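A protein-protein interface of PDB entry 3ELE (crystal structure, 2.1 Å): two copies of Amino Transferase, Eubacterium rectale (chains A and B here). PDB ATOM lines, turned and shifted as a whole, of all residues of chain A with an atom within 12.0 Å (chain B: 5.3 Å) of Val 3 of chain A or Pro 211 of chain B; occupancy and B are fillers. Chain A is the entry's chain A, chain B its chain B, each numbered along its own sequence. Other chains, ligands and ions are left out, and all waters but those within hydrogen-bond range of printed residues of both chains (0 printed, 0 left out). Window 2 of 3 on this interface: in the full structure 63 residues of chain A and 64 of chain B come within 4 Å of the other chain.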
ATOM      1  N   GLY A   1     -17.785  10.323  13.385  1.00  0.00           N
ATOM      2  CA  GLY A   1     -18.537  10.038  14.655  1.00  0.00           C
ATOM      3  C   GLY A   1     -19.796  10.875  14.880  1.00  0.00           C
ATOM      4  O   GLY A   1     -20.273  10.984  16.025  1.00  0.00           O
ATOM      5  N   MET A   2     -20.350  11.434  13.801  1.00  0.00           N
ATOM      6  CA  MET A   2     -21.551  12.274  13.863  1.00  0.00           C
ATOM      7  C   MET A   2     -22.826  11.439  13.583  1.00  0.00           C
ATOM      8  O   MET A   2     -22.934  10.743  12.545  1.00  0.00           O
ATOM      9  CB  MET A   2     -21.402  13.446  12.894  1.00  0.00           C
ATOM     10  CG  MET A   2     -22.496  14.475  12.986  1.00  0.00           C
ATOM     11  SD  MET A   2     -21.974  16.222  12.281  1.00  0.00           S
ATOM     12  CE  MET A   2     -20.730  16.647  13.585  1.00  0.00           C
ATOM     13  N   VAL A   3     -23.777  11.510  14.517  1.00  0.00           N
ATOM     14  CA  VAL A   3     -25.051  10.757  14.427  1.00  0.00           C
ATOM     15  C   VAL A   3     -26.012  11.382  13.396  1.00  0.00           C
ATOM     16  O   VAL A   3     -26.728  10.673  12.725  1.00  0.00           O
ATOM     17  CB  VAL A   3     -25.714  10.636  15.838  1.00  0.00           C
ATOM     18  CG1 VAL A   3     -27.092   9.971  15.793  1.00  0.00           C
ATOM     19  CG2 VAL A   3     -24.785   9.879  16.780  1.00  0.00           C
ATOM     20  N   VAL A   4     -26.008  12.704  13.278  1.00  0.00           N
ATOM     21  CA  VAL A   4     -26.870  13.440  12.341  1.00  0.00           C
ATOM     22  C   VAL A   4     -26.253  13.548  10.947  1.00  0.00           C
ATOM     23  O   VAL A   4     -25.080  13.239  10.749  1.00  0.00           O
ATOM     24  CB  VAL A   4     -27.160  14.873  12.847  1.00  0.00           C
ATOM     25  CG1 VAL A   4     -27.969  14.832  14.158  1.00  0.00           C
ATOM     26  CG2 VAL A   4     -25.846  15.707  13.015  1.00  0.00           C
ATOM     27  N   ASN A   5     -27.066  13.990   9.990  1.00  0.00           N
ATOM     28  CA  ASN A   5     -26.618  14.247   8.626  1.00  0.00           C
ATOM     29  C   ASN A   5     -25.661  15.451   8.662  1.00  0.00           C
ATOM     30  O   ASN A   5     -26.069  16.514   9.117  1.00  0.00           O
ATOM     31  CB  ASN A   5     -27.827  14.562   7.736  1.00  0.00           C
ATOM     32  CG  ASN A   5     -27.438  14.906   6.315  1.00  0.00           C
ATOM     33  OD1 ASN A   5     -26.991  16.008   6.060  1.00  0.00           O
ATOM     34  ND2 ASN A   5     -27.639  13.977   5.383  1.00  0.00           N
ATOM     35  N   GLU A   6     -24.424  15.283   8.181  1.00  0.00           N
ATOM     36  CA  GLU A   6     -23.424  16.384   8.209  1.00  0.00           C
ATOM     37  C   GLU A   6     -23.803  17.658   7.453  1.00  0.00           C
ATOM     38  O   GLU A   6     -23.516  18.758   7.931  1.00  0.00           O
ATOM     39  CB  GLU A   6     -22.046  15.937   7.724  1.00  0.00           C
ATOM     40  CG  GLU A   6     -21.425  14.852   8.573  1.00  0.00           C
ATOM     41  CD  GLU A   6     -19.907  14.683   8.376  1.00  0.00           C
ATOM     42  OE1 GLU A   6     -19.242  15.610   7.836  1.00  0.00           O
ATOM     43  OE2 GLU A   6     -19.387  13.621   8.807  1.00  0.00           O
ATOM     44  N   SER A   7     -24.433  17.526   6.287  1.00  0.00           N
ATOM     45  CA  SER A   7     -24.885  18.707   5.516  1.00  0.00           C
ATOM     46  C   SER A   7     -25.934  19.505   6.258  1.00  0.00           C
ATOM     47  O   SER A   7     -25.935  20.743   6.189  1.00  0.00           O
ATOM     48  CB  SER A   7     -25.462  18.316   4.159  1.00  0.00           C
ATOM     49  OG  SER A   7     -24.492  17.583   3.459  1.00  0.00           O
ATOM     50  N   MET A   8     -26.835  18.798   6.945  1.00  0.00           N
ATOM     51  CA  MET A   8     -27.873  19.447   7.739  1.00  0.00           C
ATOM     52  C   MET A   8     -27.225  20.125   8.936  1.00  0.00           C
ATOM     53  O   MET A   8     -27.507  21.278   9.189  1.00  0.00           O
ATOM     54  CB  MET A   8     -28.966  18.476   8.161  1.00  0.00           C
ATOM     55  CG  MET A   8     -29.755  17.874   6.997  1.00  0.00           C
ATOM     56  SD  MET A   8     -30.575  19.104   5.808  1.00  0.00           S
ATOM     57  CE  MET A   8     -29.149  19.449   4.523  1.00  0.00           C
ATOM     58  N   TYR A   9     -26.325  19.430   9.626  1.00  0.00           N
ATOM     59  CA  TYR A   9     -25.561  20.039  10.719  1.00  0.00           C
ATOM     60  C   TYR A   9     -24.858  21.334  10.248  1.00  0.00           C
ATOM     61  O   TYR A   9     -24.942  22.371  10.907  1.00  0.00           O
ATOM     62  CB  TYR A   9     -24.514  19.071  11.301  1.00  0.00           C
ATOM     63  CG  TYR A   9     -23.593  19.788  12.279  1.00  0.00           C
ATOM     64  CD1 TYR A   9     -23.987  20.012  13.600  1.00  0.00           C
ATOM     65  CD2 TYR A   9     -22.358  20.313  11.853  1.00  0.00           C
ATOM     66  CE1 TYR A   9     -23.166  20.693  14.484  1.00  0.00           C
ATOM     67  CE2 TYR A   9     -21.536  21.013  12.725  1.00  0.00           C
ATOM     68  CZ  TYR A   9     -21.945  21.206  14.039  1.00  0.00           C
ATOM     69  OH  TYR A   9     -21.129  21.903  14.894  1.00  0.00           O
ATOM     70  N   GLN A  10     -24.162  21.262   9.118  1.00  0.00           N
ATOM     71  CA  GLN A  10     -23.468  22.441   8.573  1.00  0.00           C
ATOM     72  C   GLN A  10     -24.403  23.576   8.193  1.00  0.00           C
ATOM     73  O   GLN A  10     -24.151  24.725   8.525  1.00  0.00           O
ATOM     74  CB  GLN A  10     -22.526  22.060   7.417  1.00  0.00           C
ATOM     75  CG  GLN A  10     -21.197  21.489   7.935  1.00  0.00           C
ATOM     76  CD  GLN A  10     -20.414  22.500   8.816  1.00  0.00           C
ATOM     77  OE1 GLN A  10     -20.436  23.712   8.570  1.00  0.00           O
ATOM     78  NE2 GLN A  10     -19.769  22.003   9.854  1.00  0.00           N
ATOM     79  N   LEU B 119     -31.698  13.473  10.842  1.00  0.00           N
ATOM     80  CA  LEU B 119     -31.085  12.233  11.266  1.00  0.00           C
ATOM     81  C   LEU B 119     -30.505  11.385  10.138  1.00  0.00           C
ATOM     82  O   LEU B 119     -29.409  10.874  10.302  1.00  0.00           O
ATOM     83  CB  LEU B 119     -32.072  11.396  12.114  1.00  0.00           C
ATOM     84  CG  LEU B 119     -32.415  11.945  13.521  1.00  0.00           C
ATOM     85  CD1 LEU B 119     -33.573  11.198  14.144  1.00  0.00           C
ATOM     86  CD2 LEU B 119     -31.214  11.964  14.516  1.00  0.00           C
ATOM     87  N   SER B 121     -28.417   9.815   7.322  1.00  0.00           N
ATOM     88  CA  SER B 121     -27.050   9.968   6.739  1.00  0.00           C
ATOM     89  C   SER B 121     -26.652   8.894   5.704  1.00  0.00           C
ATOM     90  O   SER B 121     -25.515   8.896   5.190  1.00  0.00           O
ATOM     91  CB  SER B 121     -26.018   9.997   7.881  1.00  0.00           C
ATOM     92  OG  SER B 121     -26.063   8.804   8.653  1.00  0.00           O
ATOM     93  N   THR B 173     -31.050   0.976  11.963  1.00  0.00           N
ATOM     94  CA  THR B 173     -32.166   1.549  12.696  1.00  0.00           C
ATOM     95  C   THR B 173     -31.735   2.888  13.271  1.00  0.00           C
ATOM     96  O   THR B 173     -30.798   2.925  14.054  1.00  0.00           O
ATOM     97  CB  THR B 173     -32.670   0.631  13.820  1.00  0.00           C
ATOM     98  OG1 THR B 173     -32.919  -0.663  13.280  1.00  0.00           O
ATOM     99  CG2 THR B 173     -33.971   1.173  14.433  1.00  0.00           C
ATOM    100  N   ARG B 174     -32.345   3.960  12.756  1.00  0.00           N
ATOM    101  CA  ARG B 174     -32.115   5.343  13.203  1.00  0.00           C
ATOM    102  C   ARG B 174     -33.122   5.834  14.217  1.00  0.00           C
ATOM    103  O   ARG B 174     -32.803   6.722  15.058  1.00  0.00           O
ATOM    104  CB  ARG B 174     -32.111   6.303  12.011  1.00  0.00           C
ATOM    105  CG  ARG B 174     -31.135   5.955  10.887  1.00  0.00           C
ATOM    106  CD  ARG B 174     -29.706   5.597  11.369  1.00  0.00           C
ATOM    107  NE  ARG B 174     -29.277   6.533  12.384  1.00  0.00           N
ATOM    108  CZ  ARG B 174     -28.866   7.783  12.189  1.00  0.00           C
ATOM    109  NH1 ARG B 174     -28.709   8.296  10.975  1.00  0.00           N
ATOM    110  NH2 ARG B 174     -28.548   8.518  13.260  1.00  0.00           N
ATOM    111  N   SER B 205     -29.299   0.612  21.157  1.00  0.00           N
ATOM    112  CA  SER B 205     -28.473   1.769  20.820  1.00  0.00           C
ATOM    113  C   SER B 205     -27.011   1.461  21.128  1.00  0.00           C
ATOM    114  O   SER B 205     -26.134   1.690  20.296  1.00  0.00           O
ATOM    115  CB  SER B 205     -28.919   3.011  21.599  1.00  0.00           C
ATOM    116  OG  SER B 205     -30.218   3.416  21.195  1.00  0.00           O
ATOM    117  N   GLY B 209     -23.973   0.864  18.573  1.00  0.00           N
ATOM    118  CA  GLY B 209     -22.987   1.927  18.757  1.00  0.00           C
ATOM    119  C   GLY B 209     -23.411   3.324  18.341  1.00  0.00           C
ATOM    120  O   GLY B 209     -22.572   4.174  18.044  1.00  0.00           O
ATOM    121  N   ARG B 210     -24.714   3.578  18.343  1.00  0.00           N
ATOM    122  CA  ARG B 210     -25.252   4.867  17.931  1.00  0.00           C
ATOM    123  C   ARG B 210     -26.658   5.024  18.540  1.00  0.00           C
ATOM    124  O   ARG B 210     -27.367   4.029  18.666  1.00  0.00           O
ATOM    125  CB  ARG B 210     -25.290   4.878  16.400  1.00  0.00           C
ATOM    126  CG  ARG B 210     -25.746   6.155  15.772  1.00  0.00           C
ATOM    127  CD  ARG B 210     -25.549   6.143  14.248  1.00  0.00           C
ATOM    128  NE  ARG B 210     -26.292   5.078  13.585  1.00  0.00           N
ATOM    129  CZ  ARG B 210     -26.306   4.860  12.263  1.00  0.00           C
ATOM    130  NH1 ARG B 210     -25.635   5.655  11.424  1.00  0.00           N
ATOM    131  NH2 ARG B 210     -27.027   3.846  11.773  1.00  0.00           N
ATOM    132  N   PRO B 211     -27.052   6.242  18.951  1.00  0.00           N
ATOM    133  CA  PRO B 211     -28.406   6.390  19.494  1.00  0.00           C
ATOM    134  C   PRO B 211     -29.529   6.044  18.492  1.00  0.00           C
ATOM    135  O   PRO B 211     -29.407   6.330  17.291  1.00  0.00           O
ATOM    136  CB  PRO B 211     -28.472   7.887  19.852  1.00  0.00           C
ATOM    137  CG  PRO B 211     -27.062   8.287  20.053  1.00  0.00           C
ATOM    138  CD  PRO B 211     -26.341   7.535  18.970  1.00  0.00           C
ATOM    139  N   ILE B 212     -30.552   5.353  18.986  1.00  0.00           N
ATOM    140  CA  ILE B 212     -31.780   5.096  18.237  1.00  0.00           C
ATOM    141  C   ILE B 212     -32.783   6.029  18.926  1.00  0.00           C
ATOM    142  O   ILE B 212     -33.035   5.871  20.124  1.00  0.00           O
ATOM    143  CB  ILE B 212     -32.245   3.656  18.350  1.00  0.00           C
ATOM    144  CG1 ILE B 212     -31.202   2.704  17.760  1.00  0.00           C
ATOM    145  CG2 ILE B 212     -33.576   3.459  17.634  1.00  0.00           C
ATOM    146  CD1 ILE B 212     -31.466   1.283  18.078  1.00  0.00           C
ATOM    147  N   PHE B 213     -33.323   6.993  18.182  1.00  0.00           N
ATOM    148  CA  PHE B 213     -34.304   7.942  18.720  1.00  0.00           C
ATOM    149  C   PHE B 213     -35.729   7.437  18.776  1.00  0.00           C
ATOM    150  O   PHE B 213     -36.120   6.558  18.001  1.00  0.00           O
ATOM    151  CB  PHE B 213     -34.315   9.255  17.904  1.00  0.00           C
ATOM    152  CG  PHE B 213     -33.227  10.176  18.287  1.00  0.00           C
ATOM    153  CD1 PHE B 213     -31.924   9.923  17.869  1.00  0.00           C
ATOM    154  CD2 PHE B 213     -33.483  11.280  19.106  1.00  0.00           C
ATOM    155  CE1 PHE B 213     -30.886  10.757  18.258  1.00  0.00           C
ATOM    156  CE2 PHE B 213     -32.466  12.108  19.482  1.00  0.00           C
ATOM    157  CZ  PHE B 213     -31.159  11.842  19.058  1.00  0.00           C
ATOM    158  N   TYR B 237     -36.840   8.225  28.199  1.00  0.00           N
ATOM    159  CA  TYR B 237     -35.756   7.902  27.284  1.00  0.00           C
ATOM    160  C   TYR B 237     -35.077   9.199  26.863  1.00  0.00           C
ATOM    161  O   TYR B 237     -35.733  10.129  26.395  1.00  0.00           O
ATOM    162  CB  TYR B 237     -36.338   7.153  26.076  1.00  0.00           C
ATOM    163  CG  TYR B 237     -35.319   6.600  25.106  1.00  0.00           C
ATOM    164  CD1 TYR B 237     -34.495   5.527  25.455  1.00  0.00           C
ATOM    165  CD2 TYR B 237     -35.197   7.124  23.825  1.00  0.00           C
ATOM    166  CE1 TYR B 237     -33.559   5.002  24.541  1.00  0.00           C
ATOM    167  CE2 TYR B 237     -34.278   6.607  22.921  1.00  0.00           C
ATOM    168  CZ  TYR B 237     -33.463   5.550  23.277  1.00  0.00           C
ATOM    169  OH  TYR B 237     -32.556   5.052  22.353  1.00  0.00           O
ATOM    170  N   ASN B 239     -32.902  10.057  24.373  1.00  0.00           N
ATOM    171  CA  ASN B 239     -32.884  10.408  22.968  1.00  0.00           C
ATOM    172  C   ASN B 239     -34.286  10.437  22.378  1.00  0.00           C
ATOM    173  O   ASN B 239     -34.656   9.612  21.558  1.00  0.00           O
ATOM    174  CB  ASN B 239     -31.900   9.504  22.211  1.00  0.00           C
ATOM    175  CG  ASN B 239     -30.449   9.804  22.561  1.00  0.00           C
ATOM    176  OD1 ASN B 239     -29.960  10.907  22.300  1.00  0.00           O
ATOM    177  ND2 ASN B 239     -29.739   8.819  23.107  1.00  0.00           N
ATOM    178  N   TYR B 267     -28.102  12.745  23.246  1.00  0.00           N
ATOM    179  CA  TYR B 267     -26.655  12.458  23.140  1.00  0.00           C
ATOM    180  C   TYR B 267     -25.757  13.693  22.940  1.00  0.00           C
ATOM    181  O   TYR B 267     -24.619  13.719  23.402  1.00  0.00           O
ATOM    182  CB  TYR B 267     -26.401  11.443  21.993  1.00  0.00           C
ATOM    183  CG  TYR B 267     -26.444  12.093  20.635  1.00  0.00           C
ATOM    184  CD1 TYR B 267     -27.668  12.429  20.028  1.00  0.00           C
ATOM    185  CD2 TYR B 267     -25.259  12.445  19.979  1.00  0.00           C
ATOM    186  CE1 TYR B 267     -27.705  13.076  18.789  1.00  0.00           C
ATOM    187  CE2 TYR B 267     -25.281  13.082  18.743  1.00  0.00           C
ATOM    188  CZ  TYR B 267     -26.508  13.405  18.150  1.00  0.00           C
ATOM    189  OH  TYR B 267     -26.534  14.040  16.924  1.00  0.00           O
ATOM    190  N   GLU B 271     -25.513  19.573  18.577  1.00  0.00           N
ATOM    191  CA  GLU B 271     -25.410  18.912  17.268  1.00  0.00           C
ATOM    192  C   GLU B 271     -26.788  18.578  16.681  1.00  0.00           C
ATOM    193  O   GLU B 271     -27.027  18.823  15.512  1.00  0.00           O
ATOM    194  CB  GLU B 271     -24.604  17.631  17.410  1.00  0.00           C
ATOM    195  CG  GLU B 271     -24.374  16.859  16.120  1.00  0.00           C
ATOM    196  CD  GLU B 271     -23.705  15.546  16.383  1.00  0.00           C
ATOM    197  OE1 GLU B 271     -22.564  15.552  16.816  1.00  0.00           O
ATOM    198  OE2 GLU B 271     -24.302  14.504  16.094  1.00  0.00           O
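The guanidinium group of Arg 174 of chain B sits at hydrogen-bond distance from the backbone carbonyl oxygen of Val 3 of chain A (2.9 Å).
The backbone NH (N) of Val 3 of chain A is in hydrogen-bond range of the side-chain carboxylate (OE2) of Glu 271 of chain B (3.4 Å).
OD1 of Asn 5 of chain A lies within hydrogen-bond range of N of Ser 7 of chain A, at 3.0 Å.
The side-chain amide oxygen of Asn 5 of chain A sits at hydrogen-bond distance from the backbone NH of Met 8 of chain A, 2.9 Å away.
The guanidinium group (NH1) of Arg 174 of chain B lies within hydrogen-bond range of the backbone carbonyl oxygen (O) of Leu 119 of chain B (2.8 Å).
The backbone NH (N) of Phe 213 of chain B is in hydrogen-bond range of the backbone carbonyl oxygen (O) of Arg 174 of chain B (3.2 Å).
The backbone carbonyl oxygen (O) of Ser 205 of chain B lies within hydrogen-bond range of the backbone NH (N) of Arg 210 of chain B (3.1 Å).
The side-chain hydroxyl of Tyr 267 of chain B is in hydrogen-bond range of the side-chain carboxylate of Glu 271 of chain B, 2.4 Å away.
OE2 of Glu 271 of chain B touches CG of Met 2 of chain A (3.6 Å).
Val 3 of chain A touches Leu 119 of chain B (O to O, 3.6 Å).
Val 3 of chain A touches Arg 210 of chain B.
CG2 of Val 3 of chain A touches CD of Pro 211 of chain B (3.6 Å).
Val 3 of chain A touches Tyr 267 of chain B.
Tyr 267 of chain B touches Val 4 of chain A (OH to CG1, 3.2 Å).
CG2 of Val 4 of chain A touches CG of Glu 271 of chain B, 3.6 Å away.
Leu 119 of chain B touches Asn 5 of chain A (O to N, 3.9 Å).
Glu 271 of chain B touches Tyr 9 of chain A (O to CD1, 3.8 Å).
Of the printed residues of chain B, Met 2 of chain A touches Glu 271.
Val 3 of chain A touches just these residues of chain B: Leu 119 (3.6 Å), Arg 174 (2.9 Å), Arg 210 (3.98 Å), Pro 211 (3.6 Å), Tyr 267 (3.7 Å) and Glu 271 (3.4 Å).
Printed residues of chain B within 4 Å of Val 4 of chain A: Tyr 267 and Glu 271.
Of the printed residues of chain B, Asn 5 of chain A touches Leu 119.
Ser 7 of chain A touches none of the printed residues of chain B.
Printed residues of chain B within 4 Å of Tyr 9 of chain A: Glu 271.
Leu 119 of chain B touches just these residues of chain A: Val 3 and Asn 5.
No residue of chain A comes within 4 Å of Ser 121 of chain B.
No residue of chain A comes within 4 Å of Ser 205 of chain B.
No residue of chain A comes within 4 Å of Gly 209 of chain B.
Arg 210 of chain B touches just one residue of chain A: Val 3 (3.98 Å).
Of chain A, only Val 3 comes within 4 Å of Pro 211 of chain B.
No residue of chain A comes within 4 Å of Ile 212 of chain B.
No residue of chain A comes within 4 Å of Phe 213 of chain B.
Tyr 237 of chain B touches none of the printed residues of chain A.
No residue of chain A comes within 4 Å of Asn 239 of chain B.
Of chain A, only Val 3 (3.7 Å) and Val 4 (3.2 Å) come within 4 Å of Tyr 267 of chain B.
Printed residues of chain A within 4 Å of Glu 271 of chain B: Met 2, Val 3, Val 4 and Tyr 9.
The nearest printed residue of chain B that does not touch Met 2 of chain A is Ser 121 of chain B (5.4 Å).
Printed residues of chain B that touch a printed residue of chain A: Leu 119, Arg 174, Arg 210, Pro 211, Tyr 267 and Glu 271.
Hydrophobic or aromatic side chains of chain B within 4 Å of the printed part of chain A: Pro 211 and Tyr 267.
Printed residues of chain A that touch a printed residue of chain B: Met 2, Val 3, Val 4, Asn 5 and Tyr 9.
Among the printed residues, no Asp or Glu carboxylate lies within 4 Å of a Lys or Arg side-chain nitrogen of the other chain.
No position is printed for both chains.
Of the 11 pairs that touch across the chains among the printed residues, none has its exchanged pair printed and touching as well.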
